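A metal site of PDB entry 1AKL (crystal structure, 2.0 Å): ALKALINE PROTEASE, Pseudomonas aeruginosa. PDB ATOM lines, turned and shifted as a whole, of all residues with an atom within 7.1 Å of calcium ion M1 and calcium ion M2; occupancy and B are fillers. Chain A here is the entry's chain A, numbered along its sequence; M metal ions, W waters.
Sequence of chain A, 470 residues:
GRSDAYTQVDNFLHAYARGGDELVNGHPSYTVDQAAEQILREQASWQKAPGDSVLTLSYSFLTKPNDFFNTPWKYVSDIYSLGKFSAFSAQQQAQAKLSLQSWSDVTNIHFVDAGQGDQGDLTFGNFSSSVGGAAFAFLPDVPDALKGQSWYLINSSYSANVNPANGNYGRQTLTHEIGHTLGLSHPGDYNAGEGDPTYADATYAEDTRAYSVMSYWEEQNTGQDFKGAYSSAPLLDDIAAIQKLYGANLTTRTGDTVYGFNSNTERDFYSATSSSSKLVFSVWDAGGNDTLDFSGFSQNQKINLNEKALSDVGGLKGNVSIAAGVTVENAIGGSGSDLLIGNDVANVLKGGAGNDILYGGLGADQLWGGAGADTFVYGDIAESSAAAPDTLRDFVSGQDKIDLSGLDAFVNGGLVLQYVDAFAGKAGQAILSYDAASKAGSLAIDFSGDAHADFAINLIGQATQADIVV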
ATOM      1  N   GLU A 329      18.033  29.751 -19.078  1.00  0.00           N
ATOM      2  CA  GLU A 329      19.145  29.697 -19.992  1.00  0.00           C
ATOM      3  C   GLU A 329      20.545  29.469 -19.458  1.00  0.00           C
ATOM      4  O   GLU A 329      21.327  28.800 -20.114  1.00  0.00           O
ATOM      5  CB  GLU A 329      19.175  30.943 -20.871  1.00  0.00           C
ATOM      6  CG  GLU A 329      18.078  31.029 -21.887  1.00  0.00           C
ATOM      7  CD  GLU A 329      16.755  31.453 -21.305  1.00  0.00           C
ATOM      8  OE1 GLU A 329      16.681  31.838 -20.120  1.00  0.00           O
ATOM      9  OE2 GLU A 329      15.760  31.418 -22.052  1.00  0.00           O
ATOM     10  N   ILE A 341      24.455  20.535 -16.574  1.00  0.00           N
ATOM     11  CA  ILE A 341      23.926  20.059 -17.833  1.00  0.00           C
ATOM     12  C   ILE A 341      22.884  21.036 -18.384  1.00  0.00           C
ATOM     13  O   ILE A 341      21.955  21.413 -17.680  1.00  0.00           O
ATOM     14  CB  ILE A 341      23.463  18.534 -17.773  1.00  0.00           C
ATOM     15  CG1 ILE A 341      21.951  18.382 -17.979  1.00  0.00           C
ATOM     16  CG2 ILE A 341      23.915  17.822 -16.497  1.00  0.00           C
ATOM     17  CD1 ILE A 341      21.621  17.915 -19.352  1.00  0.00           C
ATOM     18  N   GLY A 342      23.078  21.476 -19.628  1.00  0.00           N
ATOM     19  CA  GLY A 342      22.166  22.416 -20.254  1.00  0.00           C
ATOM     20  C   GLY A 342      20.975  21.771 -20.919  1.00  0.00           C
ATOM     21  O   GLY A 342      20.805  20.569 -20.898  1.00  0.00           O
ATOM     22  N   ASN A 343      20.120  22.607 -21.499  1.00  0.00           N
ATOM     23  CA  ASN A 343      18.936  22.111 -22.175  1.00  0.00           C
ATOM     24  C   ASN A 343      19.083  22.338 -23.660  1.00  0.00           C
ATOM     25  O   ASN A 343      20.187  22.638 -24.128  1.00  0.00           O
ATOM     26  CB  ASN A 343      17.672  22.773 -21.631  1.00  0.00           C
ATOM     27  CG  ASN A 343      17.765  24.280 -21.619  1.00  0.00           C
ATOM     28  OD1 ASN A 343      18.425  24.874 -22.467  1.00  0.00           O
ATOM     29  ND2 ASN A 343      17.134  24.914 -20.635  1.00  0.00           N
ATOM     30  N   ASP A 344      17.994  22.279 -24.403  1.00  0.00           N
ATOM     31  CA  ASP A 344      18.042  22.431 -25.848  1.00  0.00           C
ATOM     32  C   ASP A 344      18.480  23.776 -26.410  1.00  0.00           C
ATOM     33  O   ASP A 344      19.036  23.821 -27.508  1.00  0.00           O
ATOM     34  CB  ASP A 344      16.711  21.985 -26.473  1.00  0.00           C
ATOM     35  CG  ASP A 344      16.439  20.485 -26.282  1.00  0.00           C
ATOM     36  OD1 ASP A 344      17.341  19.759 -25.819  1.00  0.00           O
ATOM     37  OD2 ASP A 344      15.319  20.020 -26.573  1.00  0.00           O
ATOM     38  N   VAL A 345      18.241  24.861 -25.684  1.00  0.00           N
ATOM     39  CA  VAL A 345      18.629  26.178 -26.183  1.00  0.00           C
ATOM     40  C   VAL A 345      20.089  26.483 -25.907  1.00  0.00           C
ATOM     41  O   VAL A 345      20.819  25.645 -25.346  1.00  0.00           O
ATOM     42  CB  VAL A 345      17.725  27.298 -25.620  1.00  0.00           C
ATOM     43  CG1 VAL A 345      16.271  27.014 -25.917  1.00  0.00           C
ATOM     44  CG2 VAL A 345      17.946  27.469 -24.132  1.00  0.00           C
ATOM     45  N   ALA A 346      20.526  27.655 -26.352  1.00  0.00           N
ATOM     46  CA  ALA A 346      21.910  28.096 -26.163  1.00  0.00           C
ATOM     47  C   ALA A 346      22.032  28.504 -24.719  1.00  0.00           C
ATOM     48  O   ALA A 346      21.254  29.307 -24.240  1.00  0.00           O
ATOM     49  CB  ALA A 346      22.218  29.265 -27.068  1.00  0.00           C
ATOM     50  N   ASN A 347      23.039  27.968 -24.046  1.00  0.00           N
ATOM     51  CA  ASN A 347      23.206  28.234 -22.627  1.00  0.00           C
ATOM     52  C   ASN A 347      24.569  28.764 -22.318  1.00  0.00           C
ATOM     53  O   ASN A 347      25.501  28.579 -23.089  1.00  0.00           O
ATOM     54  CB  ASN A 347      23.076  26.926 -21.821  1.00  0.00           C
ATOM     55  CG  ASN A 347      21.842  26.127 -22.162  1.00  0.00           C
ATOM     56  OD1 ASN A 347      21.933  24.956 -22.584  1.00  0.00           O
ATOM     57  ND2 ASN A 347      20.677  26.729 -22.005  1.00  0.00           N
ATOM     58  N   LEU A 349      27.121  28.273 -19.395  1.00  0.00           N
ATOM     59  CA  LEU A 349      27.377  27.435 -18.238  1.00  0.00           C
ATOM     60  C   LEU A 349      28.738  27.842 -17.740  1.00  0.00           C
ATOM     61  O   LEU A 349      29.684  27.916 -18.520  1.00  0.00           O
ATOM     62  CB  LEU A 349      27.417  25.956 -18.640  1.00  0.00           C
ATOM     63  CG  LEU A 349      26.154  25.095 -18.700  1.00  0.00           C
ATOM     64  CD1 LEU A 349      24.990  25.849 -19.260  1.00  0.00           C
ATOM     65  CD2 LEU A 349      26.420  23.850 -19.526  1.00  0.00           C
ATOM     66  N   TYR A 359      28.080  19.973 -19.838  1.00  0.00           N
ATOM     67  CA  TYR A 359      27.391  19.313 -20.937  1.00  0.00           C
ATOM     68  C   TYR A 359      26.397  20.347 -21.428  1.00  0.00           C
ATOM     69  O   TYR A 359      25.431  20.656 -20.750  1.00  0.00           O
ATOM     70  CB  TYR A 359      26.668  18.067 -20.404  1.00  0.00           C
ATOM     71  CG  TYR A 359      25.973  17.217 -21.465  1.00  0.00           C
ATOM     72  CD1 TYR A 359      24.656  17.477 -21.838  1.00  0.00           C
ATOM     73  CD2 TYR A 359      26.631  16.164 -22.077  1.00  0.00           C
ATOM     74  CE1 TYR A 359      24.024  16.711 -22.791  1.00  0.00           C
ATOM     75  CE2 TYR A 359      26.005  15.388 -23.038  1.00  0.00           C
ATOM     76  CZ  TYR A 359      24.706  15.666 -23.385  1.00  0.00           C
ATOM     77  OH  TYR A 359      24.089  14.900 -24.340  1.00  0.00           O
ATOM     78  N   GLY A 360      26.651  20.912 -22.606  1.00  0.00           N
ATOM     79  CA  GLY A 360      25.752  21.930 -23.125  1.00  0.00           C
ATOM     80  C   GLY A 360      24.459  21.471 -23.771  1.00  0.00           C
ATOM     81  O   GLY A 360      23.507  22.264 -23.860  1.00  0.00           O
ATOM     82  N   GLY A 361      24.435  20.238 -24.278  1.00  0.00           N
ATOM     83  CA  GLY A 361      23.250  19.713 -24.940  1.00  0.00           C
ATOM     84  C   GLY A 361      23.087  20.388 -26.285  1.00  0.00           C
ATOM     85  O   GLY A 361      24.052  20.938 -26.827  1.00  0.00           O
ATOM     86  N   LEU A 362      21.872  20.373 -26.823  1.00  0.00           N
ATOM     87  CA  LEU A 362      21.602  21.014 -28.097  1.00  0.00           C
ATOM     88  C   LEU A 362      21.888  22.508 -28.027  1.00  0.00           C
ATOM     89  O   LEU A 362      22.104  23.067 -26.942  1.00  0.00           O
ATOM     90  CB  LEU A 362      20.159  20.781 -28.537  1.00  0.00           C
ATOM     91  CG  LEU A 362      19.789  19.326 -28.809  1.00  0.00           C
ATOM     92  CD1 LEU A 362      18.410  19.294 -29.445  1.00  0.00           C
ATOM     93  CD2 LEU A 362      20.786  18.678 -29.729  1.00  0.00           C
ATOM     94  N   GLY A 363      21.932  23.136 -29.202  1.00  0.00           N
ATOM     95  CA  GLY A 363      22.205  24.554 -29.289  1.00  0.00           C
ATOM     96  C   GLY A 363      23.681  24.920 -29.179  1.00  0.00           C
ATOM     97  O   GLY A 363      24.504  24.099 -28.723  1.00  0.00           O
ATOM     98  N   ALA A 364      23.984  26.160 -29.539  1.00  0.00           N
ATOM     99  CA  ALA A 364      25.332  26.716 -29.506  1.00  0.00           C
ATOM    100  C   ALA A 364      25.567  27.309 -28.145  1.00  0.00           C
ATOM    101  O   ALA A 364      25.181  28.441 -27.869  1.00  0.00           O
ATOM    102  CB  ALA A 364      25.482  27.777 -30.563  1.00  0.00           C
ATOM    103  N   ASP A 365      26.279  26.578 -27.299  1.00  0.00           N
ATOM    104  CA  ASP A 365      26.518  27.031 -25.957  1.00  0.00           C
ATOM    105  C   ASP A 365      27.844  27.726 -25.781  1.00  0.00           C
ATOM    106  O   ASP A 365      28.765  27.532 -26.572  1.00  0.00           O
ATOM    107  CB  ASP A 365      26.438  25.847 -25.005  1.00  0.00           C
ATOM    108  CG  ASP A 365      25.266  24.953 -25.271  1.00  0.00           C
ATOM    109  OD1 ASP A 365      24.109  25.363 -25.028  1.00  0.00           O
ATOM    110  OD2 ASP A 365      25.491  23.835 -25.732  1.00  0.00           O
ATOM    111  N   LEU A 367      30.540  27.681 -23.138  1.00  0.00           N
ATOM    112  CA  LEU A 367      30.969  26.953 -21.968  1.00  0.00           C
ATOM    113  C   LEU A 367      32.216  27.535 -21.348  1.00  0.00           C
ATOM    114  O   LEU A 367      33.204  27.755 -22.038  1.00  0.00           O
ATOM    115  CB  LEU A 367      31.213  25.491 -22.354  1.00  0.00           C
ATOM    116  CG  LEU A 367      30.025  24.515 -22.442  1.00  0.00           C
ATOM    117  CD1 LEU A 367      28.728  25.203 -22.750  1.00  0.00           C
ATOM    118  CD2 LEU A 367      30.309  23.422 -23.460  1.00  0.00           C
ATOM    119  N   TYR A 378      30.140  15.617 -24.654  1.00  0.00           N
ATOM    120  CA  TYR A 378      29.259  15.602 -25.816  1.00  0.00           C
ATOM    121  C   TYR A 378      28.750  14.184 -25.982  1.00  0.00           C
ATOM    122  O   TYR A 378      29.491  13.231 -25.746  1.00  0.00           O
ATOM    123  CB  TYR A 378      30.006  16.028 -27.095  1.00  0.00           C
ATOM    124  CG  TYR A 378      30.463  17.472 -27.057  1.00  0.00           C
ATOM    125  CD1 TYR A 378      31.585  17.830 -26.312  1.00  0.00           C
ATOM    126  CD2 TYR A 378      29.715  18.471 -27.662  1.00  0.00           C
ATOM    127  CE1 TYR A 378      31.931  19.158 -26.155  1.00  0.00           C
ATOM    128  CE2 TYR A 378      30.082  19.809 -27.515  1.00  0.00           C
ATOM    129  CZ  TYR A 378      31.183  20.137 -26.746  1.00  0.00           C
ATOM    130  OH  TYR A 378      31.517  21.455 -26.523  1.00  0.00           O
ATOM    131  N   ALA A 382      24.883  16.404 -33.126  1.00  0.00           N
ATOM    132  CA  ALA A 382      23.988  17.536 -33.307  1.00  0.00           C
ATOM    133  C   ALA A 382      24.095  18.552 -32.181  1.00  0.00           C
ATOM    134  O   ALA A 382      23.555  19.660 -32.269  1.00  0.00           O
ATOM    135  CB  ALA A 382      22.546  17.068 -33.439  1.00  0.00           C
ATOM    136  N   GLU A 383      24.804  18.189 -31.111  1.00  0.00           N
ATOM    137  CA  GLU A 383      24.966  19.081 -29.989  1.00  0.00           C
ATOM    138  C   GLU A 383      25.979  20.175 -30.274  1.00  0.00           C
ATOM    139  O   GLU A 383      26.133  21.103 -29.485  1.00  0.00           O
ATOM    140  CB  GLU A 383      25.339  18.294 -28.733  1.00  0.00           C
ATOM    141  CG  GLU A 383      24.247  17.354 -28.312  1.00  0.00           C
ATOM    142  CD  GLU A 383      24.641  16.447 -27.163  1.00  0.00           C
ATOM    143  OE1 GLU A 383      25.829  16.446 -26.757  1.00  0.00           O
ATOM    144  OE2 GLU A 383      23.739  15.744 -26.669  1.00  0.00           O
ATOM    145  N   SER A 384      26.666  20.070 -31.394  1.00  0.00           N
ATOM    146  CA  SER A 384      27.648  21.077 -31.762  1.00  0.00           C
ATOM    147  C   SER A 384      27.834  20.941 -33.270  1.00  0.00           C
ATOM    148  O   SER A 384      28.900  20.572 -33.772  1.00  0.00           O
ATOM    149  CB  SER A 384      28.950  20.842 -31.001  1.00  0.00           C
ATOM    150  OG  SER A 384      29.661  22.046 -30.790  1.00  0.00           O
ATOM    151  N   SER A 385      26.736  21.153 -33.990  1.00  0.00           N
ATOM    152  CA  SER A 385      26.749  21.067 -35.429  1.00  0.00           C
ATOM    153  C   SER A 385      27.774  22.053 -35.940  1.00  0.00           C
ATOM    154  O   SER A 385      28.230  22.924 -35.210  1.00  0.00           O
ATOM    155  CB  SER A 385      25.385  21.443 -35.979  1.00  0.00           C
ATOM    156  OG  SER A 385      25.015  22.741 -35.557  1.00  0.00           O
ATOM    157  N   ALA A 388      25.928  25.419 -36.065  1.00  0.00           N
ATOM    158  CA  ALA A 388      25.764  26.159 -34.809  1.00  0.00           C
ATOM    159  C   ALA A 388      26.637  25.534 -33.733  1.00  0.00           C
ATOM    160  O   ALA A 388      26.142  24.888 -32.809  1.00  0.00           O
ATOM    161  CB  ALA A 388      24.305  26.143 -34.391  1.00  0.00           C
ATOM    162  N   PRO A 389      27.945  25.724 -33.818  1.00  0.00           N
ATOM    163  CA  PRO A 389      28.892  25.157 -32.851  1.00  0.00           C
ATOM    164  C   PRO A 389      28.954  25.821 -31.486  1.00  0.00           C
ATOM    165  O   PRO A 389      28.604  26.982 -31.321  1.00  0.00           O
ATOM    166  CB  PRO A 389      30.220  25.286 -33.584  1.00  0.00           C
ATOM    167  CG  PRO A 389      30.060  26.581 -34.306  1.00  0.00           C
ATOM    168  CD  PRO A 389      28.663  26.459 -34.878  1.00  0.00           C
ATOM    169  N   ASP A 390      29.419  25.053 -30.499  1.00  0.00           N
ATOM    170  CA  ASP A 390      29.611  25.528 -29.143  1.00  0.00           C
ATOM    171  C   ASP A 390      30.844  26.434 -29.206  1.00  0.00           C
ATOM    172  O   ASP A 390      31.468  26.543 -30.254  1.00  0.00           O
ATOM    173  CB  ASP A 390      29.981  24.367 -28.203  1.00  0.00           C
ATOM    174  CG  ASP A 390      28.777  23.592 -27.684  1.00  0.00           C
ATOM    175  OD1 ASP A 390      27.627  23.910 -28.007  1.00  0.00           O
ATOM    176  OD2 ASP A 390      29.015  22.641 -26.913  1.00  0.00           O
HETATM  177 CA    CA M   1      25.703  22.413 -27.720  1.00  0.00          CA
HETATM  178 CA    CA M   2      22.080  23.801 -24.692  1.00  0.00          CA
HETATM  179  O   HOH W   1      26.926  21.246 -26.114  1.00  0.00           O
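Of the 25 residues printed, 6 come within 4 Å of calcium ion M1.
The nearest printed residue that does not touch calcium ion M1 is Gly 360 (4.2 Å).
Calcium ion M2 is bound by the backbone carbonyl oxygen (O) of Gly 360, the backbone carbonyl oxygen (O) of Asn 343, the backbone carbonyl oxygen (O) of Val 345, the backbone carbonyl oxygen (O) of Leu 362, the side-chain amide oxygen (OD1) of Asn 347 and the side-chain carboxylate (OD1) of Asp 365.
The side-chain hydroxyl (OH) of Tyr 359 lies within hydrogen-bond range of the side-chain carboxylate (OE2) of Glu 383, at 2.5 Å.
OH of Tyr 378 lies within hydrogen-bond range of OD2 of Asp 390.
N of Gly 363 lies within hydrogen-bond range of O of Asp 344, 3.4 Å away.
The side-chain hydroxyl (OG) of Ser 384 sits at hydrogen-bond distance from the backbone NH (N) of Asp 390, 3.0 Å away.
O of Glu 329 sits at hydrogen-bond distance from ND2 of Asn 347.
The side-chain amide oxygen (OD1) of Asn 343 sits close to the backbone NH (N) of Val 345 (3.2 Å).
Residues that only touch calcium ion M2: Asp 344 (3.99 Å).
Of the 25 residues printed, 8 come within 4 Å of calcium ion M2.
Along chain A the residues within 4 Å of calcium ion M2 span positions 343 to 365.
Water W1 bridges the side-chain carboxylate (OD2) of Asp 390 (2.6 Å) and the backbone NH (N) of Gly 361 (3.3 Å).
O of Glu 383 is bound to calcium ion M1 (2.2 Å).
O of Gly 363 binds calcium ion M1, at 2.3 Å.
Water W1 binds calcium ion M1, at 2.3 Å.
The backbone carbonyl oxygen (O) of Gly 361 is bound to calcium ion M1 (2.4 Å).
OD2 of Asp 365 binds calcium ion M1 (2.5 Å).
Calcium ion M1 is bound by OD1 of Asp 390 (2.5 Å).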
